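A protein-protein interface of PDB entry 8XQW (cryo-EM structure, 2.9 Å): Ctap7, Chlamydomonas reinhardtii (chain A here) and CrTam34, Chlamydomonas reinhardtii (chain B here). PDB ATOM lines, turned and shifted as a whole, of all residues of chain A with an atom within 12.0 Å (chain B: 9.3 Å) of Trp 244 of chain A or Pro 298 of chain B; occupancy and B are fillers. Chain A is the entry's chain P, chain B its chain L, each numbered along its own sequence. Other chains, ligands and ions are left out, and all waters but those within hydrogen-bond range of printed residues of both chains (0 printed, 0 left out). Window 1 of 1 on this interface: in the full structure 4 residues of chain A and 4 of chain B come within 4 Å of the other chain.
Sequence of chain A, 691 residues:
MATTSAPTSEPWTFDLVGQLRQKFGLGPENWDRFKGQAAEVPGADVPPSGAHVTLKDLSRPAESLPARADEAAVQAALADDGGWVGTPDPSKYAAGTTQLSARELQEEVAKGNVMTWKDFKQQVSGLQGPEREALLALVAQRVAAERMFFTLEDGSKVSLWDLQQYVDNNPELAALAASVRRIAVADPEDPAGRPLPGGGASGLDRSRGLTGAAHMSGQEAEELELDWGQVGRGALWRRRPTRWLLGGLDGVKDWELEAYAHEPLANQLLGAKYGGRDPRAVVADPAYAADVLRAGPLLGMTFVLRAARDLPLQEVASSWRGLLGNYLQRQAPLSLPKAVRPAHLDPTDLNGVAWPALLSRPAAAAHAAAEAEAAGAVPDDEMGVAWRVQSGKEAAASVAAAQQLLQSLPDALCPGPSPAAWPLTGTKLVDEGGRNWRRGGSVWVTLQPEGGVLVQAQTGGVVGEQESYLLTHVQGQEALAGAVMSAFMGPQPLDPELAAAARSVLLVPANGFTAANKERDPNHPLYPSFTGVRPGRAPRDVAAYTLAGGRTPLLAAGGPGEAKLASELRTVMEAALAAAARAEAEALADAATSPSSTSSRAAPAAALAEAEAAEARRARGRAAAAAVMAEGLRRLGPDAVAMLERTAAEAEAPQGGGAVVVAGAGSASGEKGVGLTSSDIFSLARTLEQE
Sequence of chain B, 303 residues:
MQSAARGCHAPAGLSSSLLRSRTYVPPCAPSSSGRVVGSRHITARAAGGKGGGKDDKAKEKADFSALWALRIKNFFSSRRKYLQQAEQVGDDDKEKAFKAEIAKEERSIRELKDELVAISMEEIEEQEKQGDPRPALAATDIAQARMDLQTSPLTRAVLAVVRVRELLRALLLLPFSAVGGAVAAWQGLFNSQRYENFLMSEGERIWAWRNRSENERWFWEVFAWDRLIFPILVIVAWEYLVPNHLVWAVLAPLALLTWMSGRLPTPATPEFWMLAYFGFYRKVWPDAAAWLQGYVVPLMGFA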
ATOM      1  N   ARG A 239     -26.651  -6.415  27.308  1.00  0.00           N
ATOM      2  CA  ARG A 239     -25.672  -6.531  26.234  1.00  0.00           C
ATOM      3  C   ARG A 239     -25.938  -5.406  25.252  1.00  0.00           C
ATOM      4  O   ARG A 239     -27.044  -5.313  24.716  1.00  0.00           O
ATOM      5  CB  ARG A 239     -25.782  -7.880  25.530  1.00  0.00           C
ATOM      6  CG  ARG A 239     -24.900  -8.963  26.096  1.00  0.00           C
ATOM      7  CD  ARG A 239     -25.105 -10.257  25.333  1.00  0.00           C
ATOM      8  NE  ARG A 239     -25.124 -10.017  23.896  1.00  0.00           N
ATOM      9  CZ  ARG A 239     -24.035  -9.931  23.143  1.00  0.00           C
ATOM     10  NH1 ARG A 239     -22.837 -10.072  23.691  1.00  0.00           N
ATOM     11  NH2 ARG A 239     -24.140  -9.707  21.843  1.00  0.00           N
ATOM     12  N   ARG A 240     -24.956  -4.548  25.026  1.00  0.00           N
ATOM     13  CA  ARG A 240     -25.134  -3.525  24.013  1.00  0.00           C
ATOM     14  C   ARG A 240     -25.127  -4.173  22.631  1.00  0.00           C
ATOM     15  O   ARG A 240     -24.357  -5.108  22.389  1.00  0.00           O
ATOM     16  CB  ARG A 240     -24.039  -2.468  24.113  1.00  0.00           C
ATOM     17  CG  ARG A 240     -24.143  -1.599  25.347  1.00  0.00           C
ATOM     18  CD  ARG A 240     -23.420  -0.293  25.129  1.00  0.00           C
ATOM     19  NE  ARG A 240     -23.954   0.410  23.968  1.00  0.00           N
ATOM     20  CZ  ARG A 240     -24.267   1.702  23.957  1.00  0.00           C
ATOM     21  NH1 ARG A 240     -24.089   2.442  25.042  1.00  0.00           N
ATOM     22  NH2 ARG A 240     -24.752   2.255  22.855  1.00  0.00           N
ATOM     23  N   PRO A 241     -25.969  -3.716  21.710  1.00  0.00           N
ATOM     24  CA  PRO A 241     -26.050  -4.363  20.398  1.00  0.00           C
ATOM     25  C   PRO A 241     -24.892  -3.960  19.499  1.00  0.00           C
ATOM     26  O   PRO A 241     -24.348  -2.858  19.602  1.00  0.00           O
ATOM     27  CB  PRO A 241     -27.378  -3.846  19.844  1.00  0.00           C
ATOM     28  CG  PRO A 241     -27.479  -2.482  20.423  1.00  0.00           C
ATOM     29  CD  PRO A 241     -26.858  -2.546  21.796  1.00  0.00           C
ATOM     30  N   THR A 242     -24.521  -4.871  18.605  1.00  0.00           N
ATOM     31  CA  THR A 242     -23.411  -4.660  17.686  1.00  0.00           C
ATOM     32  C   THR A 242     -23.929  -4.531  16.263  1.00  0.00           C
ATOM     33  O   THR A 242     -24.692  -5.379  15.797  1.00  0.00           O
ATOM     34  CB  THR A 242     -22.410  -5.808  17.770  1.00  0.00           C
ATOM     35  OG1 THR A 242     -23.021  -7.009  17.285  1.00  0.00           O
ATOM     36  CG2 THR A 242     -21.976  -6.014  19.198  1.00  0.00           C
ATOM     37  N   ARG A 243     -23.492  -3.477  15.573  1.00  0.00           N
ATOM     38  CA  ARG A 243     -23.882  -3.280  14.181  1.00  0.00           C
ATOM     39  C   ARG A 243     -23.556  -4.501  13.331  1.00  0.00           C
ATOM     40  O   ARG A 243     -24.267  -4.807  12.369  1.00  0.00           O
ATOM     41  CB  ARG A 243     -23.168  -2.052  13.619  1.00  0.00           C
ATOM     42  CG  ARG A 243     -23.496  -0.767  14.340  1.00  0.00           C
ATOM     43  CD  ARG A 243     -22.743   0.395  13.737  1.00  0.00           C
ATOM     44  NE  ARG A 243     -22.493   0.189  12.319  1.00  0.00           N
ATOM     45  CZ  ARG A 243     -22.523   1.157  11.413  1.00  0.00           C
ATOM     46  NH1 ARG A 243     -22.789   2.403  11.780  1.00  0.00           N
ATOM     47  NH2 ARG A 243     -22.286   0.881  10.140  1.00  0.00           N
ATOM     48  N   TRP A 244     -22.500  -5.228  13.691  1.00  0.00           N
ATOM     49  CA  TRP A 244     -21.879  -6.153  12.752  1.00  0.00           C
ATOM     50  C   TRP A 244     -22.512  -7.533  12.806  1.00  0.00           C
ATOM     51  O   TRP A 244     -22.406  -8.304  11.846  1.00  0.00           O
ATOM     52  CB  TRP A 244     -20.383  -6.209  13.027  1.00  0.00           C
ATOM     53  CG  TRP A 244     -19.836  -4.837  13.090  1.00  0.00           C
ATOM     54  CD1 TRP A 244     -19.364  -4.193  14.186  1.00  0.00           C
ATOM     55  CD2 TRP A 244     -19.751  -3.911  12.007  1.00  0.00           C
ATOM     56  NE1 TRP A 244     -18.968  -2.924  13.851  1.00  0.00           N
ATOM     57  CE2 TRP A 244     -19.197  -2.729  12.515  1.00  0.00           C
ATOM     58  CE3 TRP A 244     -20.080  -3.974  10.654  1.00  0.00           C
ATOM     59  CZ2 TRP A 244     -18.967  -1.620  11.722  1.00  0.00           C
ATOM     60  CZ3 TRP A 244     -19.849  -2.874   9.869  1.00  0.00           C
ATOM     61  CH2 TRP A 244     -19.300  -1.712  10.401  1.00  0.00           C
ATOM     62  N   LEU A 245     -23.161  -7.874  13.910  1.00  0.00           N
ATOM     63  CA  LEU A 245     -24.111  -8.972  13.856  1.00  0.00           C
ATOM     64  C   LEU A 245     -25.290  -8.549  12.993  1.00  0.00           C
ATOM     65  O   LEU A 245     -25.491  -7.360  12.729  1.00  0.00           O
ATOM     66  CB  LEU A 245     -24.581  -9.357  15.255  1.00  0.00           C
ATOM     67  CG  LEU A 245     -24.093 -10.721  15.733  1.00  0.00           C
ATOM     68  CD1 LEU A 245     -24.719 -11.073  17.065  1.00  0.00           C
ATOM     69  CD2 LEU A 245     -24.390 -11.786  14.695  1.00  0.00           C
ATOM     70  N   LEU A 246     -26.067  -9.523  12.536  1.00  0.00           N
ATOM     71  CA  LEU A 246     -27.162  -9.208  11.623  1.00  0.00           C
ATOM     72  C   LEU A 246     -28.162  -8.326  12.356  1.00  0.00           C
ATOM     73  O   LEU A 246     -28.823  -8.755  13.304  1.00  0.00           O
ATOM     74  CB  LEU A 246     -27.799 -10.482  11.078  1.00  0.00           C
ATOM     75  CG  LEU A 246     -28.475 -11.514  11.978  1.00  0.00           C
ATOM     76  CD1 LEU A 246     -29.979 -11.404  11.853  1.00  0.00           C
ATOM     77  CD2 LEU A 246     -28.015 -12.908  11.607  1.00  0.00           C
ATOM     78  N   GLY A 247     -28.234  -7.061  11.947  1.00  0.00           N
ATOM     79  CA  GLY A 247     -29.141  -6.108  12.549  1.00  0.00           C
ATOM     80  C   GLY A 247     -28.836  -5.729  13.977  1.00  0.00           C
ATOM     81  O   GLY A 247     -29.409  -4.760  14.482  1.00  0.00           O
ATOM     82  N   GLY A 248     -27.938  -6.443  14.644  1.00  0.00           N
ATOM     83  CA  GLY A 248     -27.681  -6.161  16.039  1.00  0.00           C
ATOM     84  C   GLY A 248     -28.788  -6.583  16.967  1.00  0.00           C
ATOM     85  O   GLY A 248     -29.022  -5.927  17.983  1.00  0.00           O
ATOM     86  N   LEU A 249     -29.488  -7.665  16.642  1.00  0.00           N
ATOM     87  CA  LEU A 249     -30.565  -8.159  17.489  1.00  0.00           C
ATOM     88  C   LEU A 249     -30.065  -8.829  18.759  1.00  0.00           C
ATOM     89  O   LEU A 249     -30.883  -9.170  19.620  1.00  0.00           O
ATOM     90  CB  LEU A 249     -31.445  -9.123  16.693  1.00  0.00           C
ATOM     91  CG  LEU A 249     -30.779  -9.993  15.626  1.00  0.00           C
ATOM     92  CD1 LEU A 249     -29.697 -10.900  16.194  1.00  0.00           C
ATOM     93  CD2 LEU A 249     -31.835 -10.808  14.905  1.00  0.00           C
ATOM     94  N   ASP A 250     -28.756  -9.033  18.896  1.00  0.00           N
ATOM     95  CA  ASP A 250     -28.216  -9.632  20.110  1.00  0.00           C
ATOM     96  C   ASP A 250     -28.361  -8.720  21.318  1.00  0.00           C
ATOM     97  O   ASP A 250     -28.419  -9.215  22.447  1.00  0.00           O
ATOM     98  CB  ASP A 250     -26.744  -9.978  19.899  1.00  0.00           C
ATOM     99  CG  ASP A 250     -25.925  -8.778  19.458  1.00  0.00           C
ATOM    100  OD1 ASP A 250     -26.409  -8.012  18.600  1.00  0.00           O
ATOM    101  OD2 ASP A 250     -24.804  -8.594  19.974  1.00  0.00           O
ATOM    102  N   GLY A 251     -28.434  -7.409  21.107  1.00  0.00           N
ATOM    103  CA  GLY A 251     -28.419  -6.477  22.219  1.00  0.00           C
ATOM    104  C   GLY A 251     -29.732  -6.472  22.980  1.00  0.00           C
ATOM    105  O   GLY A 251     -30.760  -6.004  22.492  1.00  0.00           O
ATOM    106  N   ALA B 290     -33.973  -3.618   0.340  1.00  0.00           N
ATOM    107  CA  ALA B 290     -33.852  -2.982   1.646  1.00  0.00           C
ATOM    108  C   ALA B 290     -33.559  -4.009   2.729  1.00  0.00           C
ATOM    109  O   ALA B 290     -32.743  -3.770   3.623  1.00  0.00           O
ATOM    110  CB  ALA B 290     -35.125  -2.204   1.967  1.00  0.00           C
ATOM    111  N   TRP B 291     -34.224  -5.161   2.665  1.00  0.00           N
ATOM    112  CA  TRP B 291     -33.970  -6.217   3.639  1.00  0.00           C
ATOM    113  C   TRP B 291     -32.503  -6.630   3.638  1.00  0.00           C
ATOM    114  O   TRP B 291     -31.883  -6.755   4.702  1.00  0.00           O
ATOM    115  CB  TRP B 291     -34.864  -7.413   3.332  1.00  0.00           C
ATOM    116  CG  TRP B 291     -34.902  -8.449   4.395  1.00  0.00           C
ATOM    117  CD1 TRP B 291     -35.819  -8.563   5.394  1.00  0.00           C
ATOM    118  CD2 TRP B 291     -33.993  -9.542   4.558  1.00  0.00           C
ATOM    119  NE1 TRP B 291     -35.534  -9.653   6.176  1.00  0.00           N
ATOM    120  CE2 TRP B 291     -34.418 -10.272   5.681  1.00  0.00           C
ATOM    121  CE3 TRP B 291     -32.860  -9.969   3.864  1.00  0.00           C
ATOM    122  CZ2 TRP B 291     -33.749 -11.405   6.127  1.00  0.00           C
ATOM    123  CZ3 TRP B 291     -32.199 -11.093   4.306  1.00  0.00           C
ATOM    124  CH2 TRP B 291     -32.643 -11.798   5.427  1.00  0.00           C
ATOM    125  N   LEU B 292     -31.927  -6.828   2.453  1.00  0.00           N
ATOM    126  CA  LEU B 292     -30.519  -7.199   2.353  1.00  0.00           C
ATOM    127  C   LEU B 292     -29.600  -6.060   2.765  1.00  0.00           C
ATOM    128  O   LEU B 292     -28.607  -6.291   3.460  1.00  0.00           O
ATOM    129  CB  LEU B 292     -30.190  -7.630   0.927  1.00  0.00           C
ATOM    130  CG  LEU B 292     -30.522  -9.061   0.518  1.00  0.00           C
ATOM    131  CD1 LEU B 292     -29.850  -9.384  -0.798  1.00  0.00           C
ATOM    132  CD2 LEU B 292     -30.099 -10.041   1.587  1.00  0.00           C
ATOM    133  N   GLN B 293     -29.900  -4.834   2.345  1.00  0.00           N
ATOM    134  CA  GLN B 293     -29.072  -3.689   2.686  1.00  0.00           C
ATOM    135  C   GLN B 293     -29.157  -3.335   4.161  1.00  0.00           C
ATOM    136  O   GLN B 293     -28.340  -2.550   4.650  1.00  0.00           O
ATOM    137  CB  GLN B 293     -29.477  -2.489   1.834  1.00  0.00           C
ATOM    138  CG  GLN B 293     -28.517  -1.334   1.868  1.00  0.00           C
ATOM    139  CD  GLN B 293     -28.933  -0.216   0.942  1.00  0.00           C
ATOM    140  OE1 GLN B 293     -28.611   0.949   1.172  1.00  0.00           O
ATOM    141  NE2 GLN B 293     -29.657  -0.566  -0.113  1.00  0.00           N
ATOM    142  N   GLY B 294     -30.124  -3.890   4.877  1.00  0.00           N
ATOM    143  CA  GLY B 294     -30.200  -3.665   6.301  1.00  0.00           C
ATOM    144  C   GLY B 294     -29.669  -4.809   7.135  1.00  0.00           C
ATOM    145  O   GLY B 294     -29.168  -4.577   8.234  1.00  0.00           O
ATOM    146  N   TYR B 295     -29.765  -6.046   6.644  1.00  0.00           N
ATOM    147  CA  TYR B 295     -29.478  -7.193   7.493  1.00  0.00           C
ATOM    148  C   TYR B 295     -28.305  -8.063   7.057  1.00  0.00           C
ATOM    149  O   TYR B 295     -27.894  -8.922   7.838  1.00  0.00           O
ATOM    150  CB  TYR B 295     -30.714  -8.097   7.611  1.00  0.00           C
ATOM    151  CG  TYR B 295     -31.780  -7.584   8.551  1.00  0.00           C
ATOM    152  CD1 TYR B 295     -31.660  -6.345   9.163  1.00  0.00           C
ATOM    153  CD2 TYR B 295     -32.906  -8.345   8.832  1.00  0.00           C
ATOM    154  CE1 TYR B 295     -32.635  -5.875  10.019  1.00  0.00           C
ATOM    155  CE2 TYR B 295     -33.884  -7.886   9.687  1.00  0.00           C
ATOM    156  CZ  TYR B 295     -33.744  -6.650  10.280  1.00  0.00           C
ATOM    157  OH  TYR B 295     -34.717  -6.189  11.133  1.00  0.00           O
ATOM    158  N   VAL B 296     -27.757  -7.884   5.857  1.00  0.00           N
ATOM    159  CA  VAL B 296     -26.760  -8.844   5.392  1.00  0.00           C
ATOM    160  C   VAL B 296     -25.438  -8.180   5.023  1.00  0.00           C
ATOM    161  O   VAL B 296     -24.395  -8.842   4.998  1.00  0.00           O
ATOM    162  CB  VAL B 296     -27.294  -9.667   4.208  1.00  0.00           C
ATOM    163  CG1 VAL B 296     -26.945  -9.002   2.891  1.00  0.00           C
ATOM    164  CG2 VAL B 296     -26.742 -11.079   4.261  1.00  0.00           C
ATOM    165  N   VAL B 297     -25.453  -6.889   4.717  1.00  0.00           N
ATOM    166  CA  VAL B 297     -24.186  -6.210   4.456  1.00  0.00           C
ATOM    167  C   VAL B 297     -23.433  -5.936   5.757  1.00  0.00           C
ATOM    168  O   VAL B 297     -22.195  -5.969   5.746  1.00  0.00           O
ATOM    169  CB  VAL B 297     -24.376  -4.935   3.618  1.00  0.00           C
ATOM    170  CG1 VAL B 297     -24.257  -5.273   2.147  1.00  0.00           C
ATOM    171  CG2 VAL B 297     -25.721  -4.318   3.863  1.00  0.00           C
ATOM    172  N   PRO B 298     -24.088  -5.660   6.895  1.00  0.00           N
ATOM    173  CA  PRO B 298     -23.323  -5.637   8.150  1.00  0.00           C
ATOM    174  C   PRO B 298     -22.701  -6.972   8.509  1.00  0.00           C
ATOM    175  O   PRO B 298     -21.758  -7.012   9.308  1.00  0.00           O
ATOM    176  CB  PRO B 298     -24.368  -5.199   9.180  1.00  0.00           C
ATOM    177  CG  PRO B 298     -25.283  -4.361   8.409  1.00  0.00           C
ATOM    178  CD  PRO B 298     -25.425  -5.075   7.103  1.00  0.00           C
ATOM    179  N   LEU B 299     -23.198  -8.078   7.951  1.00  0.00           N
ATOM    180  CA  LEU B 299     -22.536  -9.359   8.170  1.00  0.00           C
ATOM    181  C   LEU B 299     -21.246  -9.453   7.370  1.00  0.00           C
ATOM    182  O   LEU B 299     -20.490 -10.419   7.514  1.00  0.00           O
ATOM    183  CB  LEU B 299     -23.466 -10.516   7.818  1.00  0.00           C
ATOM    184  CG  LEU B 299     -24.423 -10.992   8.907  1.00  0.00           C
ATOM    185  CD1 LEU B 299     -24.740 -12.458   8.700  1.00  0.00           C
ATOM    186  CD2 LEU B 299     -23.828 -10.773  10.281  1.00  0.00           C
ATOM    187  N   MET B 300     -20.995  -8.481   6.501  1.00  0.00           N
ATOM    188  CA  MET B 300     -19.700  -8.349   5.858  1.00  0.00           C
ATOM    189  C   MET B 300     -18.998  -7.090   6.352  1.00  0.00           C
ATOM    190  O   MET B 300     -19.485  -6.374   7.228  1.00  0.00           O
ATOM    191  CB  MET B 300     -19.845  -8.319   4.340  1.00  0.00           C
ATOM    192  CG  MET B 300     -20.051  -9.687   3.721  1.00  0.00           C
ATOM    193  SD  MET B 300     -20.641  -9.585   2.024  1.00  0.00           S
ATOM    194  CE  MET B 300     -21.809 -10.936   1.991  1.00  0.00           C
ATOM    195  N   GLY B 301     -17.834  -6.821   5.771  1.00  0.00           N
ATOM    196  CA  GLY B 301     -17.032  -5.706   6.243  1.00  0.00           C
ATOM    197  C   GLY B 301     -17.599  -4.357   5.847  1.00  0.00           C
ATOM    198  O   GLY B 301     -17.657  -3.437   6.666  1.00  0.00           O
ATOM    199  N   PHE B 302     -18.015  -4.221   4.590  1.00  0.00           N
ATOM    200  CA  PHE B 302     -18.512  -2.947   4.090  1.00  0.00           C
ATOM    201  C   PHE B 302     -19.620  -2.413   4.988  1.00  0.00           C
ATOM    202  O   PHE B 302     -20.432  -3.166   5.532  1.00  0.00           O
ATOM    203  CB  PHE B 302     -19.019  -3.103   2.658  1.00  0.00           C
ATOM    204  CG  PHE B 302     -18.639  -1.970   1.751  1.00  0.00           C
ATOM    205  CD1 PHE B 302     -18.910  -0.658   2.105  1.00  0.00           C
ATOM    206  CD2 PHE B 302     -18.013  -2.213   0.538  1.00  0.00           C
ATOM    207  CE1 PHE B 302     -18.566   0.387   1.266  1.00  0.00           C
ATOM    208  CE2 PHE B 302     -17.664  -1.172  -0.304  1.00  0.00           C
ATOM    209  CZ  PHE B 302     -17.940   0.128   0.060  1.00  0.00           C
ATOM    210  N   ALA B 303     -19.634  -1.096   5.157  1.00  0.00           N
ATOM    211  CA  ALA B 303     -20.587  -0.449   6.045  1.00  0.00           C
ATOM    212  C   ALA B 303     -21.959  -0.340   5.392  1.00  0.00           C
ATOM    213  O   ALA B 303     -22.974  -0.674   6.002  1.00  0.00           O
ATOM    214  CB  ALA B 303     -20.081   0.920   6.447  1.00  0.00           C
ATOM    215  OXT ALA B 303     -22.088   0.076   4.244  1.00  0.00           O
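Of the 14 printed residues of chain B, 4 touch a printed residue of chain A.
Along chain B the printed residues that touch a printed residue of chain A span positions 295 to 301.
Of the 13 printed residues of chain A, 4 touch a printed residue of chain B.
Printed residues of chain A that touch a printed residue of chain B: Arg 243, Trp 244, Leu 245 and Leu 246.
Among the printed residues, no Asp or Glu carboxylate lies within 4 Å of a Lys or Arg side-chain nitrogen of the other chain.
Printed residues of chain B within 4 Å of Trp 244 of chain A: Pro 298, Leu 299 and Gly 301.
Of chain A, only Arg 243 (3.2 Å) and Trp 244 (2.9 Å) come within 4 Å of Pro 298 of chain B.
No residue of chain A comes within 4 Å of Val 297 of chain B.
Of the printed residues of chain A, Leu 299 of chain B touches Trp 244 (3.3 Å), Leu 245 (3.8 Å) and Leu 246 (3.4 Å).
No residue of chain A comes within 4 Å of Met 300 of chain B.
Gly 301 of chain B touches one residue of chain A.
Printed residues of chain A within 4 Å of Tyr 295 of chain B: Leu 246 (3.6 Å).
Of the printed residues of chain B, Leu 245 of chain A touches Leu 299.
Leu 249 of chain A touches none of the printed residues of chain B.
The nearest residue of chain B that does not touch Trp 244 of chain A is Met 300 of chain B (4.2 Å).
The nearest residue of chain A that does not touch Pro 298 of chain B is Leu 245 of chain A (4.3 Å).
Arg 243 of chain A touches Pro 298 of chain B.
Trp 244 of chain A touches Leu 299 of chain B.
Gly 301 of chain B touches Trp 244 of chain A.
CD2 of Leu 299 of chain B touches C of Leu 245 of chain A (3.8 Å).
Tyr 295 of chain B touches Leu 246 of chain A (O to CB, 3.6 Å).
Leu 246 of chain A touches Leu 299 of chain B.
The backbone NH (N) of Leu 245 of chain A lies close to the side-chain hydroxyl (OG1) of Thr 242 of chain A, 3.5 Å away.
O of Trp 244 of chain A lies close to O of Pro 298 of chain B (2.9 Å).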
